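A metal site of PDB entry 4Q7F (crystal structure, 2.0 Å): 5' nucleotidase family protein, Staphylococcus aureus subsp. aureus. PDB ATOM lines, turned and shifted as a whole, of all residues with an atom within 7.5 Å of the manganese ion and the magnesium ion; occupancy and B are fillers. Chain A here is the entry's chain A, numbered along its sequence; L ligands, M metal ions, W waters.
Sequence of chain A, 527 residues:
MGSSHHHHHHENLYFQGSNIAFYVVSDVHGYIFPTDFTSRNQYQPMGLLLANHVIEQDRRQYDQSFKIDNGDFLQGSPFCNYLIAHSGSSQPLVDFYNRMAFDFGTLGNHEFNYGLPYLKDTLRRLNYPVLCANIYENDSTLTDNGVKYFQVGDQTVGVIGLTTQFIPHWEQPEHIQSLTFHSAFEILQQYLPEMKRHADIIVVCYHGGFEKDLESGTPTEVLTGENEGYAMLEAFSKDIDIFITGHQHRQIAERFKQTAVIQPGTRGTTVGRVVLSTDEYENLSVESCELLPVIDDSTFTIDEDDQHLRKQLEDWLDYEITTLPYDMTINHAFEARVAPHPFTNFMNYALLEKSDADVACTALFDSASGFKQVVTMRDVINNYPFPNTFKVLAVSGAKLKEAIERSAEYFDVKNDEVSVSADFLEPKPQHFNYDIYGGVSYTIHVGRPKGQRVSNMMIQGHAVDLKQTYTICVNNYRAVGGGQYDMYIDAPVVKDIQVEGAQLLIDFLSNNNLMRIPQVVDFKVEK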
ATOM      1  N   SER A  26      16.290 -19.618  -5.215  1.00  0.00           N
ATOM      2  CA  SER A  26      16.687 -19.017  -6.481  1.00  0.00           C
ATOM      3  C   SER A  26      17.682 -19.922  -7.141  1.00  0.00           C
ATOM      4  O   SER A  26      18.432 -20.638  -6.470  1.00  0.00           O
ATOM      5  CB  SER A  26      17.329 -17.633  -6.274  1.00  0.00           C
ATOM      6  OG  SER A  26      17.560 -16.966  -7.513  1.00  0.00           O
ATOM      7  N   ASP A  27      17.666 -19.912  -8.474  1.00  0.00           N
ATOM      8  CA  ASP A  27      18.588 -20.710  -9.260  1.00  0.00           C
ATOM      9  C   ASP A  27      18.613 -22.180  -8.825  1.00  0.00           C
ATOM     10  O   ASP A  27      19.670 -22.776  -8.614  1.00  0.00           O
ATOM     11  CB  ASP A  27      19.988 -20.066  -9.222  1.00  0.00           C
ATOM     12  CG  ASP A  27      19.975 -18.599  -9.720  1.00  0.00           C
ATOM     13  OD1 ASP A  27      19.605 -17.671  -8.952  1.00  0.00           O
ATOM     14  OD2 ASP A  27      20.432 -18.356 -10.856  1.00  0.00           O
ATOM     15  N   VAL A  28      17.420 -22.747  -8.652  1.00  0.00           N
ATOM     16  CA  VAL A  28      17.274 -24.143  -8.291  1.00  0.00           C
ATOM     17  C   VAL A  28      17.829 -25.010  -9.420  1.00  0.00           C
ATOM     18  O   VAL A  28      18.432 -26.089  -9.170  1.00  0.00           O
ATOM     19  CB  VAL A  28      15.831 -24.469  -7.981  1.00  0.00           C
ATOM     20  CG1 VAL A  28      15.698 -25.950  -7.664  1.00  0.00           C
ATOM     21  CG2 VAL A  28      15.415 -23.603  -6.801  1.00  0.00           C
ATOM     22  N   HIS A  29      17.621 -24.528 -10.644  1.00  0.00           N
ATOM     23  CA  HIS A  29      18.181 -25.109 -11.855  1.00  0.00           C
ATOM     24  C   HIS A  29      17.816 -26.542 -12.132  1.00  0.00           C
ATOM     25  O   HIS A  29      18.605 -27.299 -12.696  1.00  0.00           O
ATOM     26  CB  HIS A  29      19.706 -24.928 -11.869  1.00  0.00           C
ATOM     27  CG  HIS A  29      20.158 -23.588 -12.375  1.00  0.00           C
ATOM     28  ND1 HIS A  29      19.965 -23.189 -13.672  1.00  0.00           N
ATOM     29  CD2 HIS A  29      20.845 -22.586 -11.778  1.00  0.00           C
ATOM     30  CE1 HIS A  29      20.495 -21.996 -13.855  1.00  0.00           C
ATOM     31  NE2 HIS A  29      21.027 -21.601 -12.720  1.00  0.00           N
ATOM     32  N   ASN A  70      12.874 -17.455  -7.467  1.00  0.00           N
ATOM     33  CA  ASN A  70      13.417 -16.260  -8.119  1.00  0.00           C
ATOM     34  C   ASN A  70      14.170 -16.491  -9.430  1.00  0.00           C
ATOM     35  O   ASN A  70      15.123 -15.737  -9.773  1.00  0.00           O
ATOM     36  CB  ASN A  70      14.282 -15.455  -7.138  1.00  0.00           C
ATOM     37  CG  ASN A  70      14.620 -14.056  -7.663  1.00  0.00           C
ATOM     38  OD1 ASN A  70      13.751 -13.358  -8.220  1.00  0.00           O
ATOM     39  ND2 ASN A  70      15.872 -13.631  -7.499  1.00  0.00           N
ATOM     40  N   GLY A  71      13.763 -17.516 -10.189  1.00  0.00           N
ATOM     41  CA  GLY A  71      14.347 -17.732 -11.512  1.00  0.00           C
ATOM     42  C   GLY A  71      15.402 -18.806 -11.681  1.00  0.00           C
ATOM     43  O   GLY A  71      16.024 -19.263 -10.730  1.00  0.00           O
ATOM     44  N   ASP A  72      15.609 -19.179 -12.945  1.00  0.00           N
ATOM     45  CA  ASP A  72      16.566 -20.227 -13.316  1.00  0.00           C
ATOM     46  C   ASP A  72      16.113 -21.535 -12.716  1.00  0.00           C
ATOM     47  O   ASP A  72      16.855 -22.218 -12.001  1.00  0.00           O
ATOM     48  CB  ASP A  72      18.018 -19.889 -12.927  1.00  0.00           C
ATOM     49  CG  ASP A  72      18.711 -19.007 -13.964  1.00  0.00           C
ATOM     50  OD1 ASP A  72      18.041 -18.583 -14.943  1.00  0.00           O
ATOM     51  OD2 ASP A  72      19.919 -18.731 -13.811  1.00  0.00           O
ATOM     52  N   PHE A  73      14.884 -21.895 -13.059  1.00  0.00           N
ATOM     53  CA  PHE A  73      14.263 -23.110 -12.574  1.00  0.00           C
ATOM     54  C   PHE A  73      13.985 -24.139 -13.660  1.00  0.00           C
ATOM     55  O   PHE A  73      13.722 -25.306 -13.375  1.00  0.00           O
ATOM     56  CB  PHE A  73      12.931 -22.811 -11.866  1.00  0.00           C
ATOM     57  CG  PHE A  73      11.845 -22.280 -12.781  1.00  0.00           C
ATOM     58  CD1 PHE A  73      10.975 -23.151 -13.430  1.00  0.00           C
ATOM     59  CD2 PHE A  73      11.687 -20.926 -12.979  1.00  0.00           C
ATOM     60  CE1 PHE A  73       9.998 -22.671 -14.249  1.00  0.00           C
ATOM     61  CE2 PHE A  73      10.686 -20.437 -13.779  1.00  0.00           C
ATOM     62  CZ  PHE A  73       9.846 -21.312 -14.432  1.00  0.00           C
ATOM     63  N   GLN A  75      16.026 -24.908 -16.441  1.00  0.00           N
ATOM     64  CA  GLN A  75      17.218 -25.496 -17.039  1.00  0.00           C
ATOM     65  C   GLN A  75      18.321 -25.616 -16.008  1.00  0.00           C
ATOM     66  O   GLN A  75      18.371 -24.842 -15.042  1.00  0.00           O
ATOM     67  CB  GLN A  75      17.695 -24.589 -18.192  1.00  0.00           C
ATOM     68  CG  GLN A  75      18.925 -25.081 -18.983  1.00  0.00           C
ATOM     69  CD  GLN A  75      20.258 -24.843 -18.269  1.00  0.00           C
ATOM     70  OE1 GLN A  75      20.375 -23.980 -17.392  1.00  0.00           O
ATOM     71  NE2 GLN A  75      21.275 -25.601 -18.665  1.00  0.00           N
ATOM     72  N   LEU A 107      11.369 -14.744 -13.707  1.00  0.00           N
ATOM     73  CA  LEU A 107      12.042 -15.381 -14.814  1.00  0.00           C
ATOM     74  C   LEU A 107      13.514 -15.119 -14.753  1.00  0.00           C
ATOM     75  O   LEU A 107      13.946 -13.992 -14.501  1.00  0.00           O
ATOM     76  CB  LEU A 107      11.558 -14.804 -16.151  1.00  0.00           C
ATOM     77  CG  LEU A 107      10.135 -15.074 -16.599  1.00  0.00           C
ATOM     78  CD1 LEU A 107       9.869 -14.271 -17.846  1.00  0.00           C
ATOM     79  CD2 LEU A 107       9.914 -16.560 -16.840  1.00  0.00           C
ATOM     80  N   GLY A 108      14.280 -16.189 -14.961  1.00  0.00           N
ATOM     81  CA  GLY A 108      15.720 -16.112 -15.052  1.00  0.00           C
ATOM     82  C   GLY A 108      16.096 -16.262 -16.518  1.00  0.00           C
ATOM     83  O   GLY A 108      15.249 -16.616 -17.352  1.00  0.00           O
ATOM     84  N   ASN A 109      17.357 -15.979 -16.864  1.00  0.00           N
ATOM     85  CA  ASN A 109      17.775 -16.099 -18.245  1.00  0.00           C
ATOM     86  C   ASN A 109      17.665 -17.502 -18.834  1.00  0.00           C
ATOM     87  O   ASN A 109      17.378 -17.648 -20.025  1.00  0.00           O
ATOM     88  CB  ASN A 109      19.217 -15.573 -18.441  1.00  0.00           C
ATOM     89  CG  ASN A 109      20.230 -16.277 -17.555  1.00  0.00           C
ATOM     90  OD1 ASN A 109      20.204 -16.125 -16.335  1.00  0.00           O
ATOM     91  ND2 ASN A 109      21.162 -16.991 -18.173  1.00  0.00           N
ATOM     92  N   HIS A 110      17.915 -18.521 -18.031  1.00  0.00           N
ATOM     93  CA  HIS A 110      17.855 -19.912 -18.485  1.00  0.00           C
ATOM     94  C   HIS A 110      16.457 -20.422 -18.789  1.00  0.00           C
ATOM     95  O   HIS A 110      16.296 -21.481 -19.400  1.00  0.00           O
ATOM     96  CB  HIS A 110      18.644 -20.829 -17.539  1.00  0.00           C
ATOM     97  CG  HIS A 110      20.103 -20.516 -17.513  1.00  0.00           C
ATOM     98  ND1 HIS A 110      20.943 -20.897 -18.536  1.00  0.00           N
ATOM     99  CD2 HIS A 110      20.863 -19.816 -16.641  1.00  0.00           C
ATOM    100  CE1 HIS A 110      22.173 -20.476 -18.282  1.00  0.00           C
ATOM    101  NE2 HIS A 110      22.140 -19.789 -17.151  1.00  0.00           N
ATOM    102  N   GLU A 111      15.437 -19.664 -18.379  1.00  0.00           N
ATOM    103  CA  GLU A 111      14.067 -20.006 -18.759  1.00  0.00           C
ATOM    104  C   GLU A 111      13.834 -19.913 -20.270  1.00  0.00           C
ATOM    105  O   GLU A 111      12.838 -20.446 -20.757  1.00  0.00           O
ATOM    106  CB  GLU A 111      13.047 -19.129 -18.038  1.00  0.00           C
ATOM    107  CG  GLU A 111      12.476 -19.814 -16.802  1.00  0.00           C
ATOM    108  CD  GLU A 111      13.473 -19.889 -15.667  1.00  0.00           C
ATOM    109  OE1 GLU A 111      14.046 -20.968 -15.484  1.00  0.00           O
ATOM    110  OE2 GLU A 111      13.693 -18.860 -15.015  1.00  0.00           O
ATOM    111  N   THR A 164      17.391  -9.801 -15.309  1.00  0.00           N
ATOM    112  CA  THR A 164      18.601  -9.249 -15.979  1.00  0.00           C
ATOM    113  C   THR A 164      18.322  -8.933 -17.473  1.00  0.00           C
ATOM    114  O   THR A 164      17.789  -9.778 -18.233  1.00  0.00           O
ATOM    115  CB  THR A 164      19.802 -10.190 -15.835  1.00  0.00           C
ATOM    116  OG1 THR A 164      20.952  -9.653 -16.541  1.00  0.00           O
ATOM    117  CG2 THR A 164      19.466 -11.586 -16.356  1.00  0.00           C
ATOM    118  N   TRP A 170      23.512 -13.763 -24.529  1.00  0.00           N
ATOM    119  CA  TRP A 170      23.692 -15.197 -24.282  1.00  0.00           C
ATOM    120  C   TRP A 170      22.823 -16.170 -25.077  1.00  0.00           C
ATOM    121  O   TRP A 170      23.276 -17.238 -25.491  1.00  0.00           O
ATOM    122  CB  TRP A 170      23.395 -15.517 -22.796  1.00  0.00           C
ATOM    123  CG  TRP A 170      24.097 -14.652 -21.768  1.00  0.00           C
ATOM    124  CD1 TRP A 170      25.436 -14.320 -21.748  1.00  0.00           C
ATOM    125  CD2 TRP A 170      23.521 -14.060 -20.608  1.00  0.00           C
ATOM    126  NE1 TRP A 170      25.704 -13.531 -20.650  1.00  0.00           N
ATOM    127  CE2 TRP A 170      24.542 -13.355 -19.934  1.00  0.00           C
ATOM    128  CE3 TRP A 170      22.215 -14.044 -20.064  1.00  0.00           C
ATOM    129  CZ2 TRP A 170      24.305 -12.653 -18.754  1.00  0.00           C
ATOM    130  CZ3 TRP A 170      21.998 -13.345 -18.911  1.00  0.00           C
ATOM    131  CH2 TRP A 170      23.020 -12.651 -18.272  1.00  0.00           C
ATOM    132  N   HIS A 207      15.892 -11.198 -10.743  1.00  0.00           N
ATOM    133  CA  HIS A 207      16.760 -12.266 -11.110  1.00  0.00           C
ATOM    134  C   HIS A 207      17.999 -11.602 -11.723  1.00  0.00           C
ATOM    135  O   HIS A 207      18.090 -11.476 -12.926  1.00  0.00           O
ATOM    136  CB  HIS A 207      16.173 -13.225 -12.108  1.00  0.00           C
ATOM    137  CG  HIS A 207      17.081 -14.380 -12.331  1.00  0.00           C
ATOM    138  ND1 HIS A 207      17.053 -15.493 -11.526  1.00  0.00           N
ATOM    139  CD2 HIS A 207      18.129 -14.557 -13.166  1.00  0.00           C
ATOM    140  CE1 HIS A 207      17.994 -16.334 -11.906  1.00  0.00           C
ATOM    141  NE2 HIS A 207      18.660 -15.787 -12.901  1.00  0.00           N
ATOM    142  N   GLY A 208      18.887 -11.146 -10.859  1.00  0.00           N
ATOM    143  CA  GLY A 208      20.115 -10.477 -11.231  1.00  0.00           C
ATOM    144  C   GLY A 208      20.821 -10.240  -9.912  1.00  0.00           C
ATOM    145  O   GLY A 208      20.239 -10.499  -8.833  1.00  0.00           O
ATOM    146  N   GLU A 226      24.571  -5.925 -17.019  1.00  0.00           N
ATOM    147  CA  GLU A 226      24.094  -7.291 -16.736  1.00  0.00           C
ATOM    148  C   GLU A 226      23.475  -7.322 -15.355  1.00  0.00           C
ATOM    149  O   GLU A 226      22.374  -7.848 -15.156  1.00  0.00           O
ATOM    150  CB  GLU A 226      25.253  -8.306 -16.777  1.00  0.00           C
ATOM    151  CG  GLU A 226      24.834  -9.691 -16.240  1.00  0.00           C
ATOM    152  CD  GLU A 226      25.952 -10.729 -16.222  1.00  0.00           C
ATOM    153  OE1 GLU A 226      25.706 -11.848 -15.705  1.00  0.00           O
ATOM    154  OE2 GLU A 226      27.067 -10.439 -16.705  1.00  0.00           O
ATOM    155  N   GLY A 246      19.339 -12.942  -7.312  1.00  0.00           N
ATOM    156  CA  GLY A 246      19.760 -14.286  -7.718  1.00  0.00           C
ATOM    157  C   GLY A 246      20.803 -14.149  -8.813  1.00  0.00           C
ATOM    158  O   GLY A 246      21.598 -13.192  -8.797  1.00  0.00           O
ATOM    159  N   HIS A 247      20.811 -15.104  -9.744  1.00  0.00           N
ATOM    160  CA  HIS A 247      21.649 -15.081 -10.944  1.00  0.00           C
ATOM    161  C   HIS A 247      23.134 -15.320 -10.771  1.00  0.00           C
ATOM    162  O   HIS A 247      23.737 -16.035 -11.576  1.00  0.00           O
ATOM    163  CB  HIS A 247      21.451 -13.757 -11.703  1.00  0.00           C
ATOM    164  CG  HIS A 247      22.227 -13.650 -12.971  1.00  0.00           C
ATOM    165  ND1 HIS A 247      22.011 -14.488 -14.051  1.00  0.00           N
ATOM    166  CD2 HIS A 247      23.193 -12.778 -13.366  1.00  0.00           C
ATOM    167  CE1 HIS A 247      22.813 -14.149 -15.031  1.00  0.00           C
ATOM    168  NE2 HIS A 247      23.536 -13.121 -14.649  1.00  0.00           N
ATOM    169  N   GLN A 248      23.725 -14.697  -9.750  1.00  0.00           N
ATOM    170  CA  GLN A 248      25.137 -14.845  -9.510  1.00  0.00           C
ATOM    171  C   GLN A 248      25.459 -16.068  -8.642  1.00  0.00           C
ATOM    172  O   GLN A 248      26.627 -16.410  -8.508  1.00  0.00           O
ATOM    173  CB  GLN A 248      25.699 -13.577  -8.875  1.00  0.00           C
ATOM    174  CG  GLN A 248      25.670 -12.351  -9.782  1.00  0.00           C
ATOM    175  CD  GLN A 248      26.150 -11.098  -9.036  1.00  0.00           C
ATOM    176  OE1 GLN A 248      25.746 -10.861  -7.898  1.00  0.00           O
ATOM    177  NE2 GLN A 248      27.010 -10.311  -9.672  1.00  0.00           N
ATOM    178  N   HIS A 249      24.425 -16.708  -8.048  1.00  0.00           N
ATOM    179  CA  HIS A 249      24.633 -17.899  -7.219  1.00  0.00           C
ATOM    180  C   HIS A 249      25.430 -17.607  -5.944  1.00  0.00           C
ATOM    181  O   HIS A 249      26.095 -18.484  -5.381  1.00  0.00           O
ATOM    182  CB  HIS A 249      25.328 -18.989  -8.005  1.00  0.00           C
ATOM    183  CG  HIS A 249      24.604 -19.421  -9.235  1.00  0.00           C
ATOM    184  ND1 HIS A 249      24.988 -20.511  -9.970  1.00  0.00           N
ATOM    185  CD2 HIS A 249      23.455 -18.969  -9.797  1.00  0.00           C
ATOM    186  CE1 HIS A 249      24.145 -20.669 -10.982  1.00  0.00           C
ATOM    187  NE2 HIS A 249      23.191 -19.782 -10.873  1.00  0.00           N
ATOM    188  N   GLY A 265      21.939 -18.307  -3.023  1.00  0.00           N
ATOM    189  CA  GLY A 265      22.727 -19.329  -3.668  1.00  0.00           C
ATOM    190  C   GLY A 265      22.088 -20.021  -4.868  1.00  0.00           C
ATOM    191  O   GLY A 265      21.484 -19.379  -5.754  1.00  0.00           O
ATOM    192  N   THR A 266      22.245 -21.334  -4.912  1.00  0.00           N
ATOM    193  CA  THR A 266      21.782 -22.105  -6.045  1.00  0.00           C
ATOM    194  C   THR A 266      21.623 -23.567  -5.659  1.00  0.00           C
ATOM    195  O   THR A 266      22.220 -24.043  -4.697  1.00  0.00           O
ATOM    196  CB  THR A 266      22.821 -22.013  -7.213  1.00  0.00           C
ATOM    197  OG1 THR A 266      22.351 -22.709  -8.380  1.00  0.00           O
ATOM    198  CG2 THR A 266      24.177 -22.595  -6.775  1.00  0.00           C
HETATM  199  O1  LIG L   1      26.219 -14.766 -16.812  1.00  0.00           O
HETATM  200  C1  LIG L   1      26.315 -15.883 -17.681  1.00  0.00           C
HETATM  201  C2  LIG L   1      25.163 -16.849 -17.454  1.00  0.00           C
HETATM  202  O2  LIG L   1      25.188 -17.770 -18.530  1.00  0.00           O
HETATM  203  C3  LIG L   1      25.547 -19.089 -18.095  1.00  0.00           C
HETATM  204  N1  LIG L   1      26.510 -19.686 -19.062  1.00  0.00           N
HETATM  205  C4  LIG L   1      26.091 -20.316 -20.149  1.00  0.00           C
HETATM  206  N2  LIG L   1      24.870 -20.578 -20.666  1.00  0.00           N
HETATM  207  C5  LIG L   1      24.753 -21.254 -21.836  1.00  0.00           C
HETATM  208  N3  LIG L   1      25.829 -21.687 -22.542  1.00  0.00           N
HETATM  209  C6  LIG L   1      27.100 -21.481 -22.135  1.00  0.00           C
HETATM  210  N4  LIG L   1      28.152 -21.926 -22.879  1.00  0.00           N
HETATM  211  C7  LIG L   1      27.307 -20.741 -20.868  1.00  0.00           C
HETATM  212  N5  LIG L   1      28.358 -20.332 -20.122  1.00  0.00           N
HETATM  213  C8  LIG L   1      27.868 -19.689 -19.037  1.00  0.00           C
HETATM  214  C9  LIG L   1      26.028 -18.950 -16.655  1.00  0.00           C
HETATM  215  C10 LIG L   1      25.262 -17.718 -16.213  1.00  0.00           C
HETATM  216  O3  LIG L   1      23.946 -18.135 -15.792  1.00  0.00           O
HETATM  217 MN    MN M   1      21.499 -19.403 -12.467  1.00  0.00          MN
HETATM  218 MG    MG M   2      20.708 -16.629 -14.188  1.00  0.00          MG
HETATM  219  O   HOH W   1      22.623 -17.702 -13.448  1.00  0.00           O
HETATM  220  O   HOH W   2      23.133 -20.098 -14.138  1.00  0.00           O
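A ring nitrogen (NE2) of His 110 lies within hydrogen-bond range of an oxygen (O3) of the ligand (2.8 Å). The side-chain carboxylate (OE1) of Glu 226 sits at hydrogen-bond distance from an oxygen (O1) of the ligand, at 3.2 Å.
The side-chain carboxylate (OD1) of Asp 72 is in hydrogen-bond range of the backbone NH (N) of His 110 (3.1 Å). The backbone NH (N) of Val 28 sits at hydrogen-bond distance from the backbone carbonyl oxygen (O) of Asp 72 (3.4 Å). OE2 of Glu 111 is in hydrogen-bond range of N of Asp 72, at 2.8 Å. OD1 of Asp 27 is in hydrogen-bond range of N of His 247, 2.9 Å away. The backbone carbonyl oxygen (O) of Asp 27 lies within hydrogen-bond range of the side-chain hydroxyl (OG1) of Thr 266 (2.7 Å). The side-chain hydroxyl (OG) of Ser 26 is in hydrogen-bond range of the side-chain carboxylate (OD1) of Asp 27. A ring nitrogen (ND1) of His 29 is in hydrogen-bond range of the backbone carbonyl oxygen of Gln 75, 2.7 Å away. The side-chain carboxylate (OE1) of Glu 226 is in hydrogen-bond range of a ring nitrogen (NE2) of His 247.
Four residues have an atom within 4 Å of the manganese ion: Asp 27, His 29, Asp 72 and His 249. The nearest printed residue that does not touch the manganese ion is His 247 (4.1 Å).
The manganese ion is bound by the side-chain carboxylate of Asp 72, the side-chain carboxylate of Asp 27, a ring nitrogen (NE2) of His 29, water W1, a ring nitrogen (NE2) of His 249 and water W2. The manganese ion has six donor atoms within binding distance.
The magnesium ion is bound by OD1 of Asn 109 (2.3 Å). The magnesium ion is bound by the side-chain carboxylate (OD2) of Asp 72, 2.3 Å away. The magnesium ion is bound by water W1 (2.3 Å). ND1 of His 247 binds the magnesium ion, 2.5 Å away. NE2 of His 207 is bound to the magnesium ion (2.6 Å).
Water W2 bridges an oxygen (O3) of the ligand (2.7 Å) and a ring nitrogen (NE2) of His 110 (3.2 Å). Water W1 bridges an oxygen (O3) of the ligand and the backbone carbonyl oxygen (O) of His 247.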
